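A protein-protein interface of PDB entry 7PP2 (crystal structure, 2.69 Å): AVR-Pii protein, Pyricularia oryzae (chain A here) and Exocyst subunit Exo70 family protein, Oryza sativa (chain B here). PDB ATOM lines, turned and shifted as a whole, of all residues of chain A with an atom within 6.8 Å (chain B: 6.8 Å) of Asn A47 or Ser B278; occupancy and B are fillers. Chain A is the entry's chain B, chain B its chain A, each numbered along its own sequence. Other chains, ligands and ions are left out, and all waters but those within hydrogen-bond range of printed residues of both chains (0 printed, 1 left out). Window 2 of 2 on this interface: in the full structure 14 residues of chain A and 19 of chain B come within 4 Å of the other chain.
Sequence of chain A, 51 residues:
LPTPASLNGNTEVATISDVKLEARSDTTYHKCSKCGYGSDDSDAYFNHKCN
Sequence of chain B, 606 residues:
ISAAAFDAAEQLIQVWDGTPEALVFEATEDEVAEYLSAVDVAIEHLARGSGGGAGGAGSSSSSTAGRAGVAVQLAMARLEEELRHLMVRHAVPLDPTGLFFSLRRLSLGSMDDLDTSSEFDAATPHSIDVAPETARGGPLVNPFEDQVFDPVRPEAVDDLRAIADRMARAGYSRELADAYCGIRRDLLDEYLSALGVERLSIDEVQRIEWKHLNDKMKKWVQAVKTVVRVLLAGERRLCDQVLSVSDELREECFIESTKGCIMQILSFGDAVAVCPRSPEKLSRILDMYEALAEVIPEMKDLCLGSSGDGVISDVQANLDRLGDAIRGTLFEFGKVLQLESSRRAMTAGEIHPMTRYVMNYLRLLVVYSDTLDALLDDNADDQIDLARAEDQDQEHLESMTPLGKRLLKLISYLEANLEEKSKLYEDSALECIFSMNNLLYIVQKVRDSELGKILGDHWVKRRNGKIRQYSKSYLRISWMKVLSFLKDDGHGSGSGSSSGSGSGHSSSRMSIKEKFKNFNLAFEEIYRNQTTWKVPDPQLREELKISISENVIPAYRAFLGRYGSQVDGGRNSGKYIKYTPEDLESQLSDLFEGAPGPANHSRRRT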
ATOM      1  N   SER A  42      -0.159  -3.952  25.226  1.00  0.00           N
ATOM      2  CA  SER A  42       0.274  -4.200  23.827  1.00  0.00           C
ATOM      3  C   SER A  42      -0.766  -5.064  23.105  1.00  0.00           C
ATOM      4  O   SER A  42      -1.145  -4.707  21.972  1.00  0.00           O
ATOM      5  CB  SER A  42       1.638  -4.827  23.792  1.00  0.00           C
ATOM      6  OG  SER A  42       2.587  -3.977  24.413  1.00  0.00           O
ATOM      7  N   ASP A  43      -1.216  -6.146  23.743  1.00  0.00           N
ATOM      8  CA  ASP A  43      -2.207  -7.091  23.161  1.00  0.00           C
ATOM      9  C   ASP A  43      -3.442  -6.296  22.714  1.00  0.00           C
ATOM     10  O   ASP A  43      -3.854  -6.455  21.550  1.00  0.00           O
ATOM     11  CB  ASP A  43      -2.564  -8.206  24.147  1.00  0.00           C
ATOM     12  CG  ASP A  43      -3.219  -9.402  23.482  1.00  0.00           C
ATOM     13  OD1 ASP A  43      -2.492 -10.185  22.831  1.00  0.00           O
ATOM     14  OD2 ASP A  43      -4.451  -9.533  23.608  1.00  0.00           O
ATOM     15  N   ALA A  44      -3.976  -5.448  23.599  1.00  0.00           N
ATOM     16  CA  ALA A  44      -5.155  -4.585  23.356  1.00  0.00           C
ATOM     17  C   ALA A  44      -4.869  -3.620  22.200  1.00  0.00           C
ATOM     18  O   ALA A  44      -5.787  -3.391  21.382  1.00  0.00           O
ATOM     19  CB  ALA A  44      -5.516  -3.836  24.614  1.00  0.00           C
ATOM     20  N   TYR A  45      -3.654  -3.066  22.137  1.00  0.00           N
ATOM     21  CA  TYR A  45      -3.240  -2.130  21.061  1.00  0.00           C
ATOM     22  C   TYR A  45      -3.148  -2.880  19.726  1.00  0.00           C
ATOM     23  O   TYR A  45      -3.707  -2.388  18.733  1.00  0.00           O
ATOM     24  CB  TYR A  45      -1.911  -1.428  21.348  1.00  0.00           C
ATOM     25  CG  TYR A  45      -1.451  -0.634  20.152  1.00  0.00           C
ATOM     26  CD1 TYR A  45      -2.086   0.544  19.802  1.00  0.00           C
ATOM     27  CD2 TYR A  45      -0.457  -1.107  19.309  1.00  0.00           C
ATOM     28  CE1 TYR A  45      -1.716   1.260  18.675  1.00  0.00           C
ATOM     29  CE2 TYR A  45      -0.076  -0.407  18.177  1.00  0.00           C
ATOM     30  CZ  TYR A  45      -0.709   0.780  17.858  1.00  0.00           C
ATOM     31  OH  TYR A  45      -0.345   1.483  16.747  1.00  0.00           O
ATOM     32  N   PHE A  46      -2.457  -4.023  19.700  1.00  0.00           N
ATOM     33  CA  PHE A  46      -2.077  -4.737  18.449  1.00  0.00           C
ATOM     34  C   PHE A  46      -3.303  -5.396  17.806  1.00  0.00           C
ATOM     35  O   PHE A  46      -3.224  -5.725  16.610  1.00  0.00           O
ATOM     36  CB  PHE A  46      -0.933  -5.725  18.699  1.00  0.00           C
ATOM     37  CG  PHE A  46       0.428  -5.133  18.428  1.00  0.00           C
ATOM     38  CD1 PHE A  46       0.931  -5.073  17.137  1.00  0.00           C
ATOM     39  CD2 PHE A  46       1.181  -4.586  19.454  1.00  0.00           C
ATOM     40  CE1 PHE A  46       2.167  -4.501  16.882  1.00  0.00           C
ATOM     41  CE2 PHE A  46       2.418  -4.019  19.197  1.00  0.00           C
ATOM     42  CZ  PHE A  46       2.907  -3.975  17.912  1.00  0.00           C
ATOM     43  N   ASN A  47      -4.396  -5.557  18.557  1.00  0.00           N
ATOM     44  CA  ASN A  47      -5.649  -6.199  18.074  1.00  0.00           C
ATOM     45  C   ASN A  47      -6.787  -5.175  18.042  1.00  0.00           C
ATOM     46  O   ASN A  47      -7.937  -5.597  17.841  1.00  0.00           O
ATOM     47  CB  ASN A  47      -5.983  -7.427  18.917  1.00  0.00           C
ATOM     48  CG  ASN A  47      -4.881  -8.459  18.841  1.00  0.00           C
ATOM     49  OD1 ASN A  47      -4.851  -9.275  17.923  1.00  0.00           O
ATOM     50  ND2 ASN A  47      -3.954  -8.406  19.783  1.00  0.00           N
ATOM     51  N   HIS A  48      -6.474  -3.885  18.204  1.00  0.00           N
ATOM     52  CA  HIS A  48      -7.432  -2.760  18.038  1.00  0.00           C
ATOM     53  C   HIS A  48      -7.719  -2.566  16.545  1.00  0.00           C
ATOM     54  O   HIS A  48      -6.775  -2.692  15.734  1.00  0.00           O
ATOM     55  CB  HIS A  48      -6.904  -1.470  18.686  1.00  0.00           C
ATOM     56  CG  HIS A  48      -6.294  -0.513  17.717  1.00  0.00           C
ATOM     57  ND1 HIS A  48      -5.031  -0.700  17.187  1.00  0.00           N
ATOM     58  CD2 HIS A  48      -6.771   0.627  17.172  1.00  0.00           C
ATOM     59  CE1 HIS A  48      -4.752   0.290  16.366  1.00  0.00           C
ATOM     60  NE2 HIS A  48      -5.806   1.117  16.336  1.00  0.00           N
ATOM     61  N   LYS A  49      -8.982  -2.296  16.208  1.00  0.00           N
ATOM     62  CA  LYS A  49      -9.435  -1.885  14.854  1.00  0.00           C
ATOM     63  C   LYS A  49      -9.446  -0.350  14.818  1.00  0.00           C
ATOM     64  O   LYS A  49      -9.900   0.266  15.804  1.00  0.00           O
ATOM     65  CB  LYS A  49     -10.795  -2.532  14.559  1.00  0.00           C
ATOM     66  CG  LYS A  49     -11.681  -1.825  13.539  1.00  0.00           C
ATOM     67  CD  LYS A  49     -11.340  -2.130  12.094  1.00  0.00           C
ATOM     68  CE  LYS A  49     -11.958  -1.153  11.114  1.00  0.00           C
ATOM     69  NZ  LYS A  49     -13.368  -0.839  11.452  1.00  0.00           N
ATOM     70  N   TRP B 210     -12.307 -13.512  21.848  1.00  0.00           N
ATOM     71  CA  TRP B 210     -11.113 -14.268  21.379  1.00  0.00           C
ATOM     72  C   TRP B 210     -10.861 -15.509  22.248  1.00  0.00           C
ATOM     73  O   TRP B 210     -10.544 -16.568  21.671  1.00  0.00           O
ATOM     74  CB  TRP B 210      -9.855 -13.390  21.319  1.00  0.00           C
ATOM     75  CG  TRP B 210      -8.620 -14.189  21.038  1.00  0.00           C
ATOM     76  CD1 TRP B 210      -7.484 -14.256  21.792  1.00  0.00           C
ATOM     77  CD2 TRP B 210      -8.422 -15.102  19.941  1.00  0.00           C
ATOM     78  NE1 TRP B 210      -6.585 -15.121  21.227  1.00  0.00           N
ATOM     79  CE2 TRP B 210      -7.133 -15.656  20.091  1.00  0.00           C
ATOM     80  CE3 TRP B 210      -9.198 -15.492  18.843  1.00  0.00           C
ATOM     81  CZ2 TRP B 210      -6.610 -16.571  19.180  1.00  0.00           C
ATOM     82  CZ3 TRP B 210      -8.683 -16.401  17.949  1.00  0.00           C
ATOM     83  CH2 TRP B 210      -7.405 -16.932  18.117  1.00  0.00           C
ATOM     84  N   CYS B 275     -13.172 -14.278   9.009  1.00  0.00           N
ATOM     85  CA  CYS B 275     -13.077 -13.574  10.317  1.00  0.00           C
ATOM     86  C   CYS B 275     -12.213 -12.326  10.147  1.00  0.00           C
ATOM     87  O   CYS B 275     -11.267 -12.344   9.365  1.00  0.00           O
ATOM     88  CB  CYS B 275     -12.490 -14.491  11.384  1.00  0.00           C
ATOM     89  SG  CYS B 275     -13.117 -14.161  13.051  1.00  0.00           S
ATOM     90  N   PRO B 276     -12.522 -11.198  10.828  1.00  0.00           N
ATOM     91  CA  PRO B 276     -11.654 -10.016  10.802  1.00  0.00           C
ATOM     92  C   PRO B 276     -10.209 -10.313  11.229  1.00  0.00           C
ATOM     93  O   PRO B 276     -10.022 -11.025  12.204  1.00  0.00           O
ATOM     94  CB  PRO B 276     -12.320  -9.058  11.801  1.00  0.00           C
ATOM     95  CG  PRO B 276     -13.780  -9.458  11.768  1.00  0.00           C
ATOM     96  CD  PRO B 276     -13.753 -10.965  11.603  1.00  0.00           C
ATOM     97  N   ARG B 277      -9.235  -9.763  10.493  1.00  0.00           N
ATOM     98  CA  ARG B 277      -7.783 -10.014  10.707  1.00  0.00           C
ATOM     99  C   ARG B 277      -7.372  -9.383  12.041  1.00  0.00           C
ATOM    100  O   ARG B 277      -7.576  -8.165  12.225  1.00  0.00           O
ATOM    101  CB  ARG B 277      -6.920  -9.469   9.561  1.00  0.00           C
ATOM    102  CG  ARG B 277      -7.373  -9.864   8.160  1.00  0.00           C
ATOM    103  CD  ARG B 277      -7.875 -11.290   8.015  1.00  0.00           C
ATOM    104  NE  ARG B 277      -8.158 -11.612   6.620  1.00  0.00           N
ATOM    105  CZ  ARG B 277      -8.792 -12.703   6.197  1.00  0.00           C
ATOM    106  NH1 ARG B 277      -9.233 -13.603   7.061  1.00  0.00           N
ATOM    107  NH2 ARG B 277      -8.980 -12.895   4.904  1.00  0.00           N
ATOM    108  N   SER B 278      -6.819 -10.206  12.930  1.00  0.00           N
ATOM    109  CA  SER B 278      -6.489  -9.885  14.338  1.00  0.00           C
ATOM    110  C   SER B 278      -5.218 -10.643  14.709  1.00  0.00           C
ATOM    111  O   SER B 278      -5.231 -11.871  14.766  1.00  0.00           O
ATOM    112  CB  SER B 278      -7.653 -10.242  15.222  1.00  0.00           C
ATOM    113  OG  SER B 278      -7.407  -9.861  16.564  1.00  0.00           O
ATOM    114  N   PRO B 279      -4.069  -9.954  14.909  1.00  0.00           N
ATOM    115  CA  PRO B 279      -2.803 -10.630  15.203  1.00  0.00           C
ATOM    116  C   PRO B 279      -2.914 -11.782  16.216  1.00  0.00           C
ATOM    117  O   PRO B 279      -2.267 -12.781  15.998  1.00  0.00           O
ATOM    118  CB  PRO B 279      -1.945  -9.476  15.734  1.00  0.00           C
ATOM    119  CG  PRO B 279      -2.412  -8.300  14.916  1.00  0.00           C
ATOM    120  CD  PRO B 279      -3.911  -8.492  14.827  1.00  0.00           C
ATOM    121  N   GLU B 280      -3.724 -11.617  17.266  1.00  0.00           N
ATOM    122  CA  GLU B 280      -4.140 -12.684  18.225  1.00  0.00           C
ATOM    123  C   GLU B 280      -4.148 -14.072  17.575  1.00  0.00           C
ATOM    124  O   GLU B 280      -3.696 -15.027  18.235  1.00  0.00           O
ATOM    125  CB  GLU B 280      -5.584 -12.467  18.679  1.00  0.00           C
ATOM    126  CG  GLU B 280      -5.748 -11.621  19.922  1.00  0.00           C
ATOM    127  CD  GLU B 280      -7.103 -10.942  19.973  1.00  0.00           C
ATOM    128  OE1 GLU B 280      -7.941 -11.252  19.103  1.00  0.00           O
ATOM    129  OE2 GLU B 280      -7.310 -10.100  20.868  1.00  0.00           O
ATOM    130  N   LYS B 281      -4.699 -14.175  16.360  1.00  0.00           N
ATOM    131  CA  LYS B 281      -5.212 -15.436  15.758  1.00  0.00           C
ATOM    132  C   LYS B 281      -4.147 -16.099  14.873  1.00  0.00           C
ATOM    133  O   LYS B 281      -4.336 -17.288  14.545  1.00  0.00           O
ATOM    134  CB  LYS B 281      -6.483 -15.148  14.949  1.00  0.00           C
ATOM    135  CG  LYS B 281      -7.496 -14.240  15.636  1.00  0.00           C
ATOM    136  CD  LYS B 281      -8.819 -14.092  14.912  1.00  0.00           C
ATOM    137  CE  LYS B 281      -9.807 -13.247  15.699  1.00  0.00           C
ATOM    138  NZ  LYS B 281     -10.876 -12.682  14.844  1.00  0.00           N
ATOM    139  N   LEU B 282      -3.076 -15.377  14.514  1.00  0.00           N
ATOM    140  CA  LEU B 282      -2.043 -15.823  13.536  1.00  0.00           C
ATOM    141  C   LEU B 282      -1.643 -17.282  13.798  1.00  0.00           C
ATOM    142  O   LEU B 282      -1.842 -18.112  12.891  1.00  0.00           O
ATOM    143  CB  LEU B 282      -0.819 -14.905  13.618  1.00  0.00           C
ATOM    144  CG  LEU B 282       0.301 -15.208  12.620  1.00  0.00           C
ATOM    145  CD1 LEU B 282      -0.254 -15.545  11.243  1.00  0.00           C
ATOM    146  CD2 LEU B 282       1.267 -14.040  12.517  1.00  0.00           C
ATOM    147  N   ILE B 285      -4.504 -19.888  13.106  1.00  0.00           N
ATOM    148  CA  ILE B 285      -4.820 -20.011  11.651  1.00  0.00           C
ATOM    149  C   ILE B 285      -3.761 -20.932  11.029  1.00  0.00           C
ATOM    150  O   ILE B 285      -4.152 -21.876  10.319  1.00  0.00           O
ATOM    151  CB  ILE B 285      -4.899 -18.638  10.950  1.00  0.00           C
ATOM    152  CG1 ILE B 285      -5.976 -17.734  11.559  1.00  0.00           C
ATOM    153  CG2 ILE B 285      -5.124 -18.814   9.455  1.00  0.00           C
ATOM    154  CD1 ILE B 285      -5.965 -16.314  11.025  1.00  0.00           C
ATOM    155  N   ALA B 325      -5.669 -15.481   4.681  1.00  0.00           N
ATOM    156  CA  ALA B 325      -5.970 -15.018   6.056  1.00  0.00           C
ATOM    157  C   ALA B 325      -4.670 -14.823   6.846  1.00  0.00           C
ATOM    158  O   ALA B 325      -4.641 -13.937   7.728  1.00  0.00           O
ATOM    159  CB  ALA B 325      -6.884 -16.004   6.741  1.00  0.00           C
ATOM    160  N   GLY B 328      -2.740 -11.696   5.415  1.00  0.00           N
ATOM    161  CA  GLY B 328      -3.501 -10.504   5.840  1.00  0.00           C
ATOM    162  C   GLY B 328      -3.275 -10.182   7.307  1.00  0.00           C
ATOM    163  O   GLY B 328      -3.054  -8.997   7.625  1.00  0.00           O
ATOM    164  N   THR B 329      -3.344 -11.202   8.170  1.00  0.00           N
ATOM    165  CA  THR B 329      -3.101 -11.121   9.633  1.00  0.00           C
ATOM    166  C   THR B 329      -1.704 -10.536   9.884  1.00  0.00           C
ATOM    167  O   THR B 329      -1.600  -9.513  10.592  1.00  0.00           O
ATOM    168  CB  THR B 329      -3.267 -12.505  10.272  1.00  0.00           C
ATOM    169  OG1 THR B 329      -4.602 -12.948  10.031  1.00  0.00           O
ATOM    170  CG2 THR B 329      -2.987 -12.509  11.758  1.00  0.00           C
ATOM    171  N   GLU B 332      -1.489  -6.999   8.969  1.00  0.00           N
ATOM    172  CA  GLU B 332      -2.207  -6.156   9.962  1.00  0.00           C
ATOM    173  C   GLU B 332      -1.265  -5.882  11.142  1.00  0.00           C
ATOM    174  O   GLU B 332      -1.257  -4.743  11.637  1.00  0.00           O
ATOM    175  CB  GLU B 332      -3.510  -6.837  10.391  1.00  0.00           C
ATOM    176  CG  GLU B 332      -4.430  -5.964  11.232  1.00  0.00           C
ATOM    177  CD  GLU B 332      -5.043  -4.760  10.533  1.00  0.00           C
ATOM    178  OE1 GLU B 332      -5.151  -4.772   9.284  1.00  0.00           O
ATOM    179  OE2 GLU B 332      -5.414  -3.804  11.246  1.00  0.00           O
ATOM    180  N   VAL B 336      -0.179  -2.135  12.067  1.00  0.00           N
ATOM    181  CA  VAL B 336      -0.483  -1.585  13.423  1.00  0.00           C
ATOM    182  C   VAL B 336       0.824  -1.171  14.116  1.00  0.00           C
ATOM    183  O   VAL B 336       0.800  -0.174  14.857  1.00  0.00           O
ATOM    184  CB  VAL B 336      -1.295  -2.600  14.253  1.00  0.00           C
ATOM    185  CG1 VAL B 336      -1.330  -2.259  15.735  1.00  0.00           C
ATOM    186  CG2 VAL B 336      -2.710  -2.738  13.713  1.00  0.00           C
ATOM    187  N   TYR B 357       6.153  -7.517  23.564  1.00  0.00           N
ATOM    188  CA  TYR B 357       5.063  -8.104  22.741  1.00  0.00           C
ATOM    189  C   TYR B 357       5.588  -8.438  21.342  1.00  0.00           C
ATOM    190  O   TYR B 357       5.406  -9.597  20.900  1.00  0.00           O
ATOM    191  CB  TYR B 357       3.853  -7.173  22.643  1.00  0.00           C
ATOM    192  CG  TYR B 357       2.710  -7.759  21.850  1.00  0.00           C
ATOM    193  CD1 TYR B 357       1.761  -8.560  22.460  1.00  0.00           C
ATOM    194  CD2 TYR B 357       2.597  -7.547  20.486  1.00  0.00           C
ATOM    195  CE1 TYR B 357       0.717  -9.118  21.740  1.00  0.00           C
ATOM    196  CE2 TYR B 357       1.561  -8.100  19.749  1.00  0.00           C
ATOM    197  CZ  TYR B 357       0.615  -8.889  20.378  1.00  0.00           C
ATOM    198  OH  TYR B 357      -0.416  -9.443  19.672  1.00  0.00           O
ATOM    199  N   TYR B 361       6.164 -12.195  19.727  1.00  0.00           N
ATOM    200  CA  TYR B 361       5.409 -12.486  18.481  1.00  0.00           C
ATOM    201  C   TYR B 361       6.360 -13.077  17.433  1.00  0.00           C
ATOM    202  O   TYR B 361       6.098 -14.189  16.954  1.00  0.00           O
ATOM    203  CB  TYR B 361       4.731 -11.209  17.978  1.00  0.00           C
ATOM    204  CG  TYR B 361       3.542 -11.409  17.074  1.00  0.00           C
ATOM    205  CD1 TYR B 361       2.286 -11.685  17.594  1.00  0.00           C
ATOM    206  CD2 TYR B 361       3.661 -11.275  15.699  1.00  0.00           C
ATOM    207  CE1 TYR B 361       1.184 -11.848  16.772  1.00  0.00           C
ATOM    208  CE2 TYR B 361       2.567 -11.430  14.862  1.00  0.00           C
ATOM    209  CZ  TYR B 361       1.325 -11.717  15.401  1.00  0.00           C
ATOM    210  OH  TYR B 361       0.249 -11.873  14.579  1.00  0.00           O
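The side-chain hydroxyl of Ser B278 lies within hydrogen-bond range of the side-chain amide oxygen of Asn A47 (3.0 Å). The backbone nitrogen of Pro B279 lies close to the side-chain amide oxygen of Asn A47, 3.2 Å away. The backbone carbonyl oxygen (O) of Val B336 sits at hydrogen-bond distance from the side-chain hydroxyl (OH) of Tyr A45. OD1 of Asn A47 is in hydrogen-bond range of N of Glu B280, 2.7 Å away.
The side-chain amide nitrogen of Asn A47 sits at hydrogen-bond distance from the backbone carbonyl oxygen of Asp A43 (2.6 Å). The backbone carbonyl oxygen (O) of Tyr A45 lies within hydrogen-bond range of a ring nitrogen (ND1) of His A48. The side-chain hydroxyl (OH) of Tyr B361 lies within hydrogen-bond range of the backbone carbonyl oxygen (O) of Pro B279 (3.0 Å). The side-chain hydroxyl (OG) of Ser B278 is in hydrogen-bond range of the side-chain carboxylate (OE1) of Glu B280 (2.9 Å).
CB of Ser A42 touches CB of Tyr B357, at 3.4 Å. OD1 of Asp A43 touches CE1 of Tyr B357, 3.6 Å away. Phe A46 touches Pro B279 (O to CG, 3.2 Å). Phe A46 touches Val B336 (CA to CG1, 3.8 Å). CG of Phe A46 touches CE2 of Tyr B357 (3.4 Å). Asn A47 touches Tyr B357.
Printed residues of chain B within 4 Å of Ser A42: Tyr B357. Of the printed residues of chain B, Asp A43 touches Tyr B357. Asn A47 touches four residues of chain B. Ser B278 touches just one residue of chain A: Asn A47. Of the printed residues of chain A, Pro B279 touches Phe A46 (3.2 Å) and Asn A47 (3.2 Å). Printed residues of chain A within 4 Å of Val B336: Tyr A45 (2.8 Å) and Phe A46 (3.8 Å). Of the printed residues of chain A, Tyr B357 touches Ser A42 (3.4 Å), Asp A43 (3.6 Å), Phe A46 (3.4 Å) and Asn A47 (3.7 Å). The nearest residue of chain B that does not touch Asn A47 is Lys B281 (5.1 Å). The nearest printed residue of chain A that does not touch Pro B279 is His A48 (6.3 Å).
Hydrophobic or aromatic side chains of chain B within 4 Å of the printed part of chain A: Pro B279, Val B336 and Tyr B357. Printed residues of chain A that touch a printed residue of chain B: Ser A42, Asp A43, Tyr A45, Phe A46 and Asn A47. Hydrophobic or aromatic side chains of chain A that line the printed part of chain B: Tyr A45 and Phe A46. Among the printed residues, 10 pairs touch across the chains.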
